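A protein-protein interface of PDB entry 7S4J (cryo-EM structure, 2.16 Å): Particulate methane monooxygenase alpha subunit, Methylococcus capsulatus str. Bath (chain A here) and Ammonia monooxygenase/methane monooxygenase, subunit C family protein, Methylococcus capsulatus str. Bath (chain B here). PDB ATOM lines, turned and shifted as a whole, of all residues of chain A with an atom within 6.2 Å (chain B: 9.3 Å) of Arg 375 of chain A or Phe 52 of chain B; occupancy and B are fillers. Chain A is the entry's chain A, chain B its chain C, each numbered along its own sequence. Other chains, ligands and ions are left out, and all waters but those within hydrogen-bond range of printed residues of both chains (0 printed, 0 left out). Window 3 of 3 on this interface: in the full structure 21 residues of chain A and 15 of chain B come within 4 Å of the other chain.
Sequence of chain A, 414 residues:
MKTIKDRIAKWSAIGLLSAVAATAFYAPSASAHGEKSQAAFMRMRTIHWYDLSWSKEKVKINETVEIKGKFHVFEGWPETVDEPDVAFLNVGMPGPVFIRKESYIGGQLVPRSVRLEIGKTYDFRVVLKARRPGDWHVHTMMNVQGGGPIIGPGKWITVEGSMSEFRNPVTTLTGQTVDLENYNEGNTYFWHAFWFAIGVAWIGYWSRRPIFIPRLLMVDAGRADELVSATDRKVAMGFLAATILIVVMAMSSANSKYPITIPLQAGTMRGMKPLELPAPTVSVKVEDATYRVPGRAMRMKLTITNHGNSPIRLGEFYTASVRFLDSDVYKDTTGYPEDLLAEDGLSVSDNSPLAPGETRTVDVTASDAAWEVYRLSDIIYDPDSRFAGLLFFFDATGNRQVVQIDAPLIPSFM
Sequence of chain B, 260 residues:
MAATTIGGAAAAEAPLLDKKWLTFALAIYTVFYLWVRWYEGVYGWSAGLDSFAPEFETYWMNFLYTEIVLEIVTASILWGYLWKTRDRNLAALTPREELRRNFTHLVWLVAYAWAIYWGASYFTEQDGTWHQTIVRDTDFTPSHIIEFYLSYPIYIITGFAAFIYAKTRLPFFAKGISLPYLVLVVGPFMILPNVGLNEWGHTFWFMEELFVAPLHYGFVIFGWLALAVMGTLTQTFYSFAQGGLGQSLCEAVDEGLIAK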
ATOM      1  N   GLU A  35      17.718  -5.054   0.423  1.00  0.00           N
ATOM      2  CA  GLU A  35      16.859  -4.406  -0.547  1.00  0.00           C
ATOM      3  C   GLU A  35      17.256  -4.887  -1.945  1.00  0.00           C
ATOM      4  O   GLU A  35      18.094  -5.789  -2.085  1.00  0.00           O
ATOM      5  CB  GLU A  35      16.933  -2.885  -0.375  1.00  0.00           C
ATOM      6  CG  GLU A  35      18.154  -2.216  -0.980  1.00  0.00           C
ATOM      7  CD  GLU A  35      19.429  -2.504  -0.220  1.00  0.00           C
ATOM      8  OE1 GLU A  35      19.358  -3.090   0.879  1.00  0.00           O
ATOM      9  OE2 GLU A  35      20.510  -2.140  -0.722  1.00  0.00           O
ATOM     10  N   LYS A  36      16.631  -4.304  -2.969  1.00  0.00           N
ATOM     11  CA  LYS A  36      16.693  -4.745  -4.360  1.00  0.00           C
ATOM     12  C   LYS A  36      15.901  -6.031  -4.543  1.00  0.00           C
ATOM     13  O   LYS A  36      15.629  -6.443  -5.672  1.00  0.00           O
ATOM     14  CB  LYS A  36      18.131  -4.957  -4.846  1.00  0.00           C
ATOM     15  CG  LYS A  36      19.012  -3.732  -4.833  1.00  0.00           C
ATOM     16  CD  LYS A  36      20.458  -4.142  -4.664  1.00  0.00           C
ATOM     17  CE  LYS A  36      21.401  -3.108  -5.228  1.00  0.00           C
ATOM     18  NZ  LYS A  36      22.223  -3.680  -6.320  1.00  0.00           N
ATOM     19  N   SER A  37      15.490  -6.652  -3.442  1.00  0.00           N
ATOM     20  CA  SER A  37      14.688  -7.862  -3.537  1.00  0.00           C
ATOM     21  C   SER A  37      13.252  -7.617  -3.111  1.00  0.00           C
ATOM     22  O   SER A  37      12.348  -8.321  -3.569  1.00  0.00           O
ATOM     23  CB  SER A  37      15.302  -8.973  -2.690  1.00  0.00           C
ATOM     24  OG  SER A  37      16.078  -9.843  -3.490  1.00  0.00           O
ATOM     25  N   GLN A  38      13.023  -6.638  -2.245  1.00  0.00           N
ATOM     26  CA  GLN A  38      11.665  -6.311  -1.855  1.00  0.00           C
ATOM     27  C   GLN A  38      10.923  -5.650  -3.009  1.00  0.00           C
ATOM     28  O   GLN A  38      11.521  -5.114  -3.943  1.00  0.00           O
ATOM     29  CB  GLN A  38      11.652  -5.397  -0.634  1.00  0.00           C
ATOM     30  CG  GLN A  38      12.798  -5.613   0.315  1.00  0.00           C
ATOM     31  CD  GLN A  38      12.679  -4.755   1.550  1.00  0.00           C
ATOM     32  OE1 GLN A  38      13.222  -3.654   1.608  1.00  0.00           O
ATOM     33  NE2 GLN A  38      11.963  -5.252   2.548  1.00  0.00           N
ATOM     34  N   ALA A  40       9.196  -3.157  -5.333  1.00  0.00           N
ATOM     35  CA  ALA A  40       9.536  -1.764  -5.588  1.00  0.00           C
ATOM     36  C   ALA A  40       8.462  -0.824  -5.062  1.00  0.00           C
ATOM     37  O   ALA A  40       8.775   0.225  -4.493  1.00  0.00           O
ATOM     38  CB  ALA A  40       9.752  -1.545  -7.084  1.00  0.00           C
ATOM     39  N   ARG A  43       8.772  -0.565  -1.344  1.00  0.00           N
ATOM     40  CA  ARG A  43       9.916   0.272  -1.001  1.00  0.00           C
ATOM     41  C   ARG A  43       9.612   1.742  -1.248  1.00  0.00           C
ATOM     42  O   ARG A  43      10.126   2.612  -0.539  1.00  0.00           O
ATOM     43  CB  ARG A  43      11.147  -0.160  -1.795  1.00  0.00           C
ATOM     44  CG  ARG A  43      11.815  -1.404  -1.254  1.00  0.00           C
ATOM     45  CD  ARG A  43      13.160  -1.642  -1.897  1.00  0.00           C
ATOM     46  NE  ARG A  43      13.033  -2.303  -3.188  1.00  0.00           N
ATOM     47  CZ  ARG A  43      13.727  -1.973  -4.267  1.00  0.00           C
ATOM     48  NH1 ARG A  43      14.607  -0.987  -4.247  1.00  0.00           N
ATOM     49  NH2 ARG A  43      13.538  -2.653  -5.392  1.00  0.00           N
ATOM     50  N   ALA A 370      20.789   3.941 -11.213  1.00  0.00           N
ATOM     51  CA  ALA A 370      20.238   3.427  -9.968  1.00  0.00           C
ATOM     52  C   ALA A 370      18.836   2.867 -10.136  1.00  0.00           C
ATOM     53  O   ALA A 370      18.497   1.896  -9.456  1.00  0.00           O
ATOM     54  CB  ALA A 370      20.222   4.521  -8.901  1.00  0.00           C
ATOM     55  N   TRP A 371      18.031   3.437 -11.032  1.00  0.00           N
ATOM     56  CA  TRP A 371      16.687   2.947 -11.293  1.00  0.00           C
ATOM     57  C   TRP A 371      16.665   1.481 -11.699  1.00  0.00           C
ATOM     58  O   TRP A 371      15.711   0.776 -11.361  1.00  0.00           O
ATOM     59  CB  TRP A 371      16.027   3.800 -12.380  1.00  0.00           C
ATOM     60  CG  TRP A 371      14.690   3.301 -12.821  1.00  0.00           C
ATOM     61  CD1 TRP A 371      14.437   2.391 -13.801  1.00  0.00           C
ATOM     62  CD2 TRP A 371      13.419   3.680 -12.286  1.00  0.00           C
ATOM     63  NE1 TRP A 371      13.086   2.182 -13.914  1.00  0.00           N
ATOM     64  CE2 TRP A 371      12.438   2.961 -12.993  1.00  0.00           C
ATOM     65  CE3 TRP A 371      13.015   4.559 -11.279  1.00  0.00           C
ATOM     66  CZ2 TRP A 371      11.080   3.093 -12.727  1.00  0.00           C
ATOM     67  CZ3 TRP A 371      11.666   4.688 -11.014  1.00  0.00           C
ATOM     68  CH2 TRP A 371      10.715   3.960 -11.735  1.00  0.00           C
ATOM     69  N   GLU A 372      17.690   1.009 -12.396  1.00  0.00           N
ATOM     70  CA  GLU A 372      17.809  -0.394 -12.754  1.00  0.00           C
ATOM     71  C   GLU A 372      18.702  -1.182 -11.811  1.00  0.00           C
ATOM     72  O   GLU A 372      18.465  -2.374 -11.616  1.00  0.00           O
ATOM     73  CB  GLU A 372      18.344  -0.530 -14.186  1.00  0.00           C
ATOM     74  CG  GLU A 372      17.253  -0.601 -15.239  1.00  0.00           C
ATOM     75  CD  GLU A 372      17.789  -0.917 -16.619  1.00  0.00           C
ATOM     76  OE1 GLU A 372      18.963  -0.594 -16.892  1.00  0.00           O
ATOM     77  OE2 GLU A 372      17.033  -1.488 -17.434  1.00  0.00           O
ATOM     78  N   VAL A 373      19.714  -0.548 -11.216  1.00  0.00           N
ATOM     79  CA  VAL A 373      20.598  -1.246 -10.290  1.00  0.00           C
ATOM     80  C   VAL A 373      19.848  -1.654  -9.030  1.00  0.00           C
ATOM     81  O   VAL A 373      20.007  -2.778  -8.540  1.00  0.00           O
ATOM     82  CB  VAL A 373      21.819  -0.368  -9.964  1.00  0.00           C
ATOM     83  CG1 VAL A 373      22.521  -0.865  -8.712  1.00  0.00           C
ATOM     84  CG2 VAL A 373      22.775  -0.339 -11.142  1.00  0.00           C
ATOM     85  N   TYR A 374      19.019  -0.766  -8.487  1.00  0.00           N
ATOM     86  CA  TYR A 374      18.223  -1.062  -7.309  1.00  0.00           C
ATOM     87  C   TYR A 374      16.861  -1.631  -7.675  1.00  0.00           C
ATOM     88  O   TYR A 374      15.995  -1.765  -6.805  1.00  0.00           O
ATOM     89  CB  TYR A 374      18.095   0.191  -6.446  1.00  0.00           C
ATOM     90  CG  TYR A 374      19.318   0.390  -5.589  1.00  0.00           C
ATOM     91  CD1 TYR A 374      20.431   1.053  -6.084  1.00  0.00           C
ATOM     92  CD2 TYR A 374      19.375  -0.115  -4.300  1.00  0.00           C
ATOM     93  CE1 TYR A 374      21.560   1.218  -5.314  1.00  0.00           C
ATOM     94  CE2 TYR A 374      20.497   0.049  -3.522  1.00  0.00           C
ATOM     95  CZ  TYR A 374      21.588   0.717  -4.035  1.00  0.00           C
ATOM     96  OH  TYR A 374      22.709   0.883  -3.258  1.00  0.00           O
ATOM     97  N   ARG A 375      16.669  -1.971  -8.948  1.00  0.00           N
ATOM     98  CA  ARG A 375      15.500  -2.705  -9.422  1.00  0.00           C
ATOM     99  C   ARG A 375      14.205  -1.970  -9.098  1.00  0.00           C
ATOM    100  O   ARG A 375      13.190  -2.565  -8.738  1.00  0.00           O
ATOM    101  CB  ARG A 375      15.491  -4.127  -8.865  1.00  0.00           C
ATOM    102  CG  ARG A 375      16.845  -4.801  -8.934  1.00  0.00           C
ATOM    103  CD  ARG A 375      16.755  -6.257  -8.541  1.00  0.00           C
ATOM    104  NE  ARG A 375      16.122  -7.084  -9.562  1.00  0.00           N
ATOM    105  CZ  ARG A 375      16.631  -7.331 -10.763  1.00  0.00           C
ATOM    106  NH1 ARG A 375      17.809  -6.852 -11.130  1.00  0.00           N
ATOM    107  NH2 ARG A 375      15.945  -8.088 -11.614  1.00  0.00           N
ATOM    108  N   LEU A 376      14.256  -0.648  -9.227  1.00  0.00           N
ATOM    109  CA  LEU A 376      13.047   0.158  -9.224  1.00  0.00           C
ATOM    110  C   LEU A 376      12.197  -0.099 -10.456  1.00  0.00           C
ATOM    111  O   LEU A 376      10.987   0.142 -10.420  1.00  0.00           O
ATOM    112  CB  LEU A 376      13.416   1.637  -9.139  1.00  0.00           C
ATOM    113  CG  LEU A 376      13.259   2.297  -7.772  1.00  0.00           C
ATOM    114  CD1 LEU A 376      14.171   1.633  -6.773  1.00  0.00           C
ATOM    115  CD2 LEU A 376      13.577   3.774  -7.859  1.00  0.00           C
ATOM    116  N   SER A 377      12.800  -0.597 -11.531  1.00  0.00           N
ATOM    117  CA  SER A 377      12.090  -1.004 -12.731  1.00  0.00           C
ATOM    118  C   SER A 377      11.344  -2.316 -12.546  1.00  0.00           C
ATOM    119  O   SER A 377      10.553  -2.694 -13.413  1.00  0.00           O
ATOM    120  CB  SER A 377      13.068  -1.122 -13.899  1.00  0.00           C
ATOM    121  OG  SER A 377      14.077  -2.074 -13.614  1.00  0.00           O
ATOM    122  N   ASP A 378      11.573  -3.014 -11.434  1.00  0.00           N
ATOM    123  CA  ASP A 378      10.896  -4.267 -11.134  1.00  0.00           C
ATOM    124  C   ASP A 378       9.486  -4.044 -10.600  1.00  0.00           C
ATOM    125  O   ASP A 378       8.827  -4.994 -10.170  1.00  0.00           O
ATOM    126  CB  ASP A 378      11.716  -5.090 -10.141  1.00  0.00           C
ATOM    127  CG  ASP A 378      12.738  -5.975 -10.824  1.00  0.00           C
ATOM    128  OD1 ASP A 378      12.841  -5.921 -12.066  1.00  0.00           O
ATOM    129  OD2 ASP A 378      13.440  -6.730 -10.118  1.00  0.00           O
ATOM    130  N   ILE A 379       9.010  -2.796 -10.617  1.00  0.00           N
ATOM    131  CA  ILE A 379       7.627  -2.507 -10.258  1.00  0.00           C
ATOM    132  C   ILE A 379       6.644  -3.115 -11.248  1.00  0.00           C
ATOM    133  O   ILE A 379       5.486  -3.362 -10.884  1.00  0.00           O
ATOM    134  CB  ILE A 379       7.419  -0.982 -10.134  1.00  0.00           C
ATOM    135  CG1 ILE A 379       6.024  -0.659  -9.593  1.00  0.00           C
ATOM    136  CG2 ILE A 379       7.651  -0.298 -11.465  1.00  0.00           C
ATOM    137  CD1 ILE A 379       5.977   0.556  -8.710  1.00  0.00           C
ATOM    138  N   TYR A 381       6.585  -6.032 -12.129  1.00  0.00           N
ATOM    139  CA  TYR A 381       6.256  -7.332 -11.571  1.00  0.00           C
ATOM    140  C   TYR A 381       5.300  -7.235 -10.391  1.00  0.00           C
ATOM    141  O   TYR A 381       4.746  -8.255  -9.972  1.00  0.00           O
ATOM    142  CB  TYR A 381       7.548  -8.036 -11.154  1.00  0.00           C
ATOM    143  CG  TYR A 381       8.479  -8.378 -12.287  1.00  0.00           C
ATOM    144  CD1 TYR A 381       8.341  -9.569 -12.980  1.00  0.00           C
ATOM    145  CD2 TYR A 381       9.503  -7.514 -12.660  1.00  0.00           C
ATOM    146  CE1 TYR A 381       9.183  -9.888 -14.018  1.00  0.00           C
ATOM    147  CE2 TYR A 381      10.359  -7.831 -13.696  1.00  0.00           C
ATOM    148  CZ  TYR A 381      10.195  -9.023 -14.364  1.00  0.00           C
ATOM    149  OH  TYR A 381      11.027  -9.354 -15.400  1.00  0.00           O
ATOM    150  N   ALA B  47      31.418 -11.311  -1.828  1.00  0.00           N
ATOM    151  CA  ALA B  47      30.844 -12.245  -2.806  1.00  0.00           C
ATOM    152  C   ALA B  47      29.989 -13.316  -2.140  1.00  0.00           C
ATOM    153  O   ALA B  47      30.373 -14.478  -2.025  1.00  0.00           O
ATOM    154  CB  ALA B  47      31.921 -12.882  -3.690  1.00  0.00           C
ATOM    155  N   GLY B  48      28.794 -12.903  -1.718  1.00  0.00           N
ATOM    156  CA  GLY B  48      27.867 -13.763  -1.012  1.00  0.00           C
ATOM    157  C   GLY B  48      26.886 -13.040  -0.112  1.00  0.00           C
ATOM    158  O   GLY B  48      25.926 -13.650   0.363  1.00  0.00           O
ATOM    159  N   LEU B  49      27.088 -11.744   0.121  1.00  0.00           N
ATOM    160  CA  LEU B  49      26.058 -10.957   0.794  1.00  0.00           C
ATOM    161  C   LEU B  49      25.020 -10.436  -0.195  1.00  0.00           C
ATOM    162  O   LEU B  49      23.813 -10.501   0.064  1.00  0.00           O
ATOM    163  CB  LEU B  49      26.686  -9.801   1.572  1.00  0.00           C
ATOM    164  CG  LEU B  49      27.794 -10.172   2.551  1.00  0.00           C
ATOM    165  CD1 LEU B  49      28.531  -8.937   3.033  1.00  0.00           C
ATOM    166  CD2 LEU B  49      27.217 -10.945   3.724  1.00  0.00           C
ATOM    167  N   ASP B  50      25.472  -9.905  -1.327  1.00  0.00           N
ATOM    168  CA  ASP B  50      24.568  -9.354  -2.330  1.00  0.00           C
ATOM    169  C   ASP B  50      24.268 -10.411  -3.385  1.00  0.00           C
ATOM    170  O   ASP B  50      25.168 -10.841  -4.110  1.00  0.00           O
ATOM    171  CB  ASP B  50      25.180  -8.113  -2.975  1.00  0.00           C
ATOM    172  CG  ASP B  50      24.170  -7.309  -3.769  1.00  0.00           C
ATOM    173  OD1 ASP B  50      22.983  -7.692  -3.792  1.00  0.00           O
ATOM    174  OD2 ASP B  50      24.565  -6.292  -4.374  1.00  0.00           O
ATOM    175  N   SER B  51      23.003 -10.812  -3.480  1.00  0.00           N
ATOM    176  CA  SER B  51      22.590 -11.846  -4.419  1.00  0.00           C
ATOM    177  C   SER B  51      22.471 -11.341  -5.851  1.00  0.00           C
ATOM    178  O   SER B  51      22.433 -12.158  -6.775  1.00  0.00           O
ATOM    179  CB  SER B  51      21.256 -12.450  -3.976  1.00  0.00           C
ATOM    180  OG  SER B  51      20.178 -11.907  -4.714  1.00  0.00           O
ATOM    181  N   PHE B  52      22.406 -10.028  -6.060  1.00  0.00           N
ATOM    182  CA  PHE B  52      22.297  -9.462  -7.396  1.00  0.00           C
ATOM    183  C   PHE B  52      23.641  -9.032  -7.963  1.00  0.00           C
ATOM    184  O   PHE B  52      23.698  -8.582  -9.112  1.00  0.00           O
ATOM    185  CB  PHE B  52      21.327  -8.276  -7.384  1.00  0.00           C
ATOM    186  CG  PHE B  52      19.886  -8.684  -7.349  1.00  0.00           C
ATOM    187  CD1 PHE B  52      19.260  -9.165  -8.484  1.00  0.00           C
ATOM    188  CD2 PHE B  52      19.163  -8.612  -6.173  1.00  0.00           C
ATOM    189  CE1 PHE B  52      17.938  -9.553  -8.449  1.00  0.00           C
ATOM    190  CE2 PHE B  52      17.841  -8.999  -6.132  1.00  0.00           C
ATOM    191  CZ  PHE B  52      17.228  -9.469  -7.271  1.00  0.00           C
ATOM    192  N   ALA B  53      24.715  -9.162  -7.197  1.00  0.00           N
ATOM    193  CA  ALA B  53      26.050  -8.845  -7.667  1.00  0.00           C
ATOM    194  C   ALA B  53      26.573  -9.954  -8.573  1.00  0.00           C
ATOM    195  O   ALA B  53      26.197 -11.119  -8.426  1.00  0.00           O
ATOM    196  CB  ALA B  53      26.984  -8.647  -6.478  1.00  0.00           C
ATOM    197  N   PRO B  54      27.447  -9.621  -9.528  1.00  0.00           N
ATOM    198  CA  PRO B  54      27.975 -10.669 -10.409  1.00  0.00           C
ATOM    199  C   PRO B  54      28.948 -11.617  -9.730  1.00  0.00           C
ATOM    200  O   PRO B  54      29.079 -12.763 -10.176  1.00  0.00           O
ATOM    201  CB  PRO B  54      28.636  -9.853 -11.522  1.00  0.00           C
ATOM    202  CG  PRO B  54      29.232  -8.715 -10.774  1.00  0.00           C
ATOM    203  CD  PRO B  54      28.163  -8.348  -9.739  1.00  0.00           C
ATOM    204  N   GLU B  55      29.632 -11.192  -8.667  1.00  0.00           N
ATOM    205  CA  GLU B  55      30.502 -12.104  -7.934  1.00  0.00           C
ATOM    206  C   GLU B  55      29.725 -13.193  -7.206  1.00  0.00           C
ATOM    207  O   GLU B  55      30.226 -14.317  -7.071  1.00  0.00           O
ATOM    208  CB  GLU B  55      31.377 -11.325  -6.948  1.00  0.00           C
ATOM    209  CG  GLU B  55      30.602 -10.501  -5.936  1.00  0.00           C
ATOM    210  CD  GLU B  55      30.417  -9.063  -6.374  1.00  0.00           C
ATOM    211  OE1 GLU B  55      30.434  -8.804  -7.596  1.00  0.00           O
ATOM    212  OE2 GLU B  55      30.250  -8.191  -5.496  1.00  0.00           O
ATOM    213  N   PHE B  56      28.512 -12.891  -6.747  1.00  0.00           N
ATOM    214  CA  PHE B  56      27.654 -13.928  -6.198  1.00  0.00           C
ATOM    215  C   PHE B  56      27.316 -14.977  -7.245  1.00  0.00           C
ATOM    216  O   PHE B  56      27.329 -16.172  -6.941  1.00  0.00           O
ATOM    217  CB  PHE B  56      26.377 -13.305  -5.634  1.00  0.00           C
ATOM    218  CG  PHE B  56      25.363 -14.306  -5.158  1.00  0.00           C
ATOM    219  CD1 PHE B  56      25.398 -14.775  -3.857  1.00  0.00           C
ATOM    220  CD2 PHE B  56      24.372 -14.772  -6.003  1.00  0.00           C
ATOM    221  CE1 PHE B  56      24.469 -15.689  -3.412  1.00  0.00           C
ATOM    222  CE2 PHE B  56      23.441 -15.688  -5.559  1.00  0.00           C
ATOM    223  CZ  PHE B  56      23.490 -16.146  -4.263  1.00  0.00           C
ATOM    224  N   GLU B  57      27.032 -14.558  -8.476  1.00  0.00           N
ATOM    225  CA  GLU B  57      26.683 -15.492  -9.536  1.00  0.00           C
ATOM    226  C   GLU B  57      27.804 -16.467  -9.863  1.00  0.00           C
ATOM    227  O   GLU B  57      27.516 -17.593 -10.278  1.00  0.00           O
ATOM    228  CB  GLU B  57      26.282 -14.728 -10.799  1.00  0.00           C
ATOM    229  CG  GLU B  57      24.901 -15.086 -11.319  1.00  0.00           C
ATOM    230  CD  GLU B  57      24.889 -16.382 -12.102  1.00  0.00           C
ATOM    231  OE1 GLU B  57      25.958 -16.781 -12.610  1.00  0.00           O
ATOM    232  OE2 GLU B  57      23.809 -17.001 -12.213  1.00  0.00           O
ATOM    233  N   THR B  58      29.065 -16.076  -9.681  1.00  0.00           N
ATOM    234  CA  THR B  58      30.177 -16.980  -9.939  1.00  0.00           C
ATOM    235  C   THR B  58      30.636 -17.748  -8.712  1.00  0.00           C
ATOM    236  O   THR B  58      31.225 -18.822  -8.864  1.00  0.00           O
ATOM    237  CB  THR B  58      31.380 -16.220 -10.514  1.00  0.00           C
ATOM    238  OG1 THR B  58      32.583 -16.940 -10.223  1.00  0.00           O
ATOM    239  CG2 THR B  58      31.483 -14.845  -9.919  1.00  0.00           C
ATOM    240  N   MET B  61      26.009 -19.177  -7.201  1.00  0.00           N
ATOM    241  CA  MET B  61      25.083 -19.769  -8.162  1.00  0.00           C
ATOM    242  C   MET B  61      25.754 -20.894  -8.939  1.00  0.00           C
ATOM    243  O   MET B  61      25.134 -21.933  -9.206  1.00  0.00           O
ATOM    244  CB  MET B  61      24.547 -18.696  -9.107  1.00  0.00           C
ATOM    245  CG  MET B  61      23.531 -17.764  -8.469  1.00  0.00           C
ATOM    246  SD  MET B  61      22.203 -18.605  -7.584  1.00  0.00           S
ATOM    247  CE  MET B  61      21.451 -19.554  -8.898  1.00  0.00           C
ATOM    248  N   ARG B 136      17.072 -11.391   3.917  1.00  0.00           N
ATOM    249  CA  ARG B 136      17.103 -12.311   2.786  1.00  0.00           C
ATOM    250  C   ARG B 136      16.871 -11.571   1.475  1.00  0.00           C
ATOM    251  O   ARG B 136      16.057 -10.648   1.390  1.00  0.00           O
ATOM    252  CB  ARG B 136      16.047 -13.410   2.938  1.00  0.00           C
ATOM    253  CG  ARG B 136      15.747 -13.847   4.350  1.00  0.00           C
ATOM    254  CD  ARG B 136      14.356 -14.449   4.410  1.00  0.00           C
ATOM    255  NE  ARG B 136      14.204 -15.425   5.483  1.00  0.00           N
ATOM    256  CZ  ARG B 136      14.681 -16.661   5.446  1.00  0.00           C
ATOM    257  NH1 ARG B 136      15.356 -17.113   4.402  1.00  0.00           N
ATOM    258  NH2 ARG B 136      14.469 -17.468   6.482  1.00  0.00           N
ATOM    259  N   ASP B 137      17.602 -11.994   0.440  1.00  0.00           N
ATOM    260  CA  ASP B 137      17.422 -11.447  -0.898  1.00  0.00           C
ATOM    261  C   ASP B 137      16.785 -12.453  -1.846  1.00  0.00           C
ATOM    262  O   ASP B 137      16.371 -12.066  -2.946  1.00  0.00           O
ATOM    263  CB  ASP B 137      18.756 -10.987  -1.489  1.00  0.00           C
ATOM    264  CG  ASP B 137      19.185  -9.643  -0.969  1.00  0.00           C
ATOM    265  OD1 ASP B 137      19.153  -9.460   0.263  1.00  0.00           O
ATOM    266  OD2 ASP B 137      19.545  -8.770  -1.786  1.00  0.00           O
ATOM    267  N   THR B 138      16.699 -13.722  -1.455  1.00  0.00           N
ATOM    268  CA  THR B 138      16.243 -14.782  -2.344  1.00  0.00           C
ATOM    269  C   THR B 138      16.107 -16.099  -1.595  1.00  0.00           C
ATOM    270  O   THR B 138      16.403 -16.181  -0.399  1.00  0.00           O
ATOM    271  CB  THR B 138      17.209 -14.942  -3.522  1.00  0.00           C
ATOM    272  OG1 THR B 138      16.669 -15.869  -4.472  1.00  0.00           O
ATOM    273  CG2 THR B 138      18.573 -15.407  -3.044  1.00  0.00           C
ATOM    274  N   ASP B 139      15.646 -17.131  -2.297  1.00  0.00           N
ATOM    275  CA  ASP B 139      15.639 -18.484  -1.774  1.00  0.00           C
ATOM    276  C   ASP B 139      16.987 -19.174  -1.910  1.00  0.00           C
ATOM    277  O   ASP B 139      17.147 -20.288  -1.401  1.00  0.00           O
ATOM    278  CB  ASP B 139      14.565 -19.320  -2.486  1.00  0.00           C
ATOM    279  CG  ASP B 139      13.245 -18.582  -2.618  1.00  0.00           C
ATOM    280  OD1 ASP B 139      12.685 -18.163  -1.584  1.00  0.00           O
ATOM    281  OD2 ASP B 139      12.772 -18.413  -3.761  1.00  0.00           O
ATOM    282  N   PHE B 140      17.952 -18.548  -2.580  1.00  0.00           N
ATOM    283  CA  PHE B 140      19.268 -19.129  -2.833  1.00  0.00           C
ATOM    284  C   PHE B 140      20.383 -18.334  -2.169  1.00  0.00           C
ATOM    285  O   PHE B 140      21.401 -18.027  -2.793  1.00  0.00           O
ATOM    286  CB  PHE B 140      19.514 -19.261  -4.335  1.00  0.00           C
ATOM    287  CG  PHE B 140      18.374 -19.894  -5.079  1.00  0.00           C
ATOM    288  CD1 PHE B 140      18.204 -21.267  -5.066  1.00  0.00           C
ATOM    289  CD2 PHE B 140      17.461 -19.120  -5.772  1.00  0.00           C
ATOM    290  CE1 PHE B 140      17.156 -21.856  -5.740  1.00  0.00           C
ATOM    291  CE2 PHE B 140      16.409 -19.704  -6.449  1.00  0.00           C
ATOM    292  CZ  PHE B 140      16.256 -21.074  -6.433  1.00  0.00           C
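Of the 17 printed residues of chain A, 4 touch a printed residue of chain B.
Along chain A the printed residues that touch a printed residue of chain B span positions 35 to 375.
Along chain B the printed residues that touch a printed residue of chain A span positions 52 to 137.
The side-chain amino group (NZ) of Lys 36 of chain A sits at hydrogen-bond distance from the backbone carbonyl oxygen (O) of Val 373 of chain A.
The guanidinium group of Arg 43 of chain A lies within hydrogen-bond range of the backbone carbonyl oxygen of Arg 375 of chain A, 3.4 Å away.
The guanidinium group of Arg 375 of chain A is in salt-bridge range of the side-chain carboxylate of Asp 378 of chain A.
N of Phe 52 of chain B sits close to OD1 of Asp 50 of chain B.
The backbone carbonyl oxygen (O) of Glu 35 of chain A lies close to the side-chain carboxylate (OD2) of Asp 137 of chain B, 3.3 Å away.
The backbone carbonyl oxygen (O) of Asp 137 of chain B lies close to the side-chain hydroxyl (OG) of Ser 37 of chain A (2.3 Å).
Among the printed residues, merely in contact across the chains: Lys 36 of chain A with Phe 52 of chain B (3.4 Å), Ser 37 of chain A with Phe 52 of chain B (3.3 Å) and Arg 375 of chain A with Phe 52 of chain B (3.3 Å).
Of the printed residues of chain B, Glu 35 of chain A touches Asp 137.
Printed residues of chain B within 4 Å of Lys 36 of chain A: Phe 52.
Arg 43 of chain A touches none of the printed residues of chain B.
Arg 375 of chain A touches just one residue of chain B: Phe 52.
No residue of chain B comes within 4 Å of Asp 378 of chain A.
Phe 52 of chain B touches just these residues of chain A: Lys 36, Ser 37 and Arg 375.
Ala 53 of chain B touches none of the printed residues of chain A.
The nearest residue of chain B that does not touch Arg 375 of chain A is Ser 51 of chain B (7.6 Å).
The nearest residue of chain A that does not touch Phe 52 of chain B is Glu 35 of chain A (5.1 Å).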
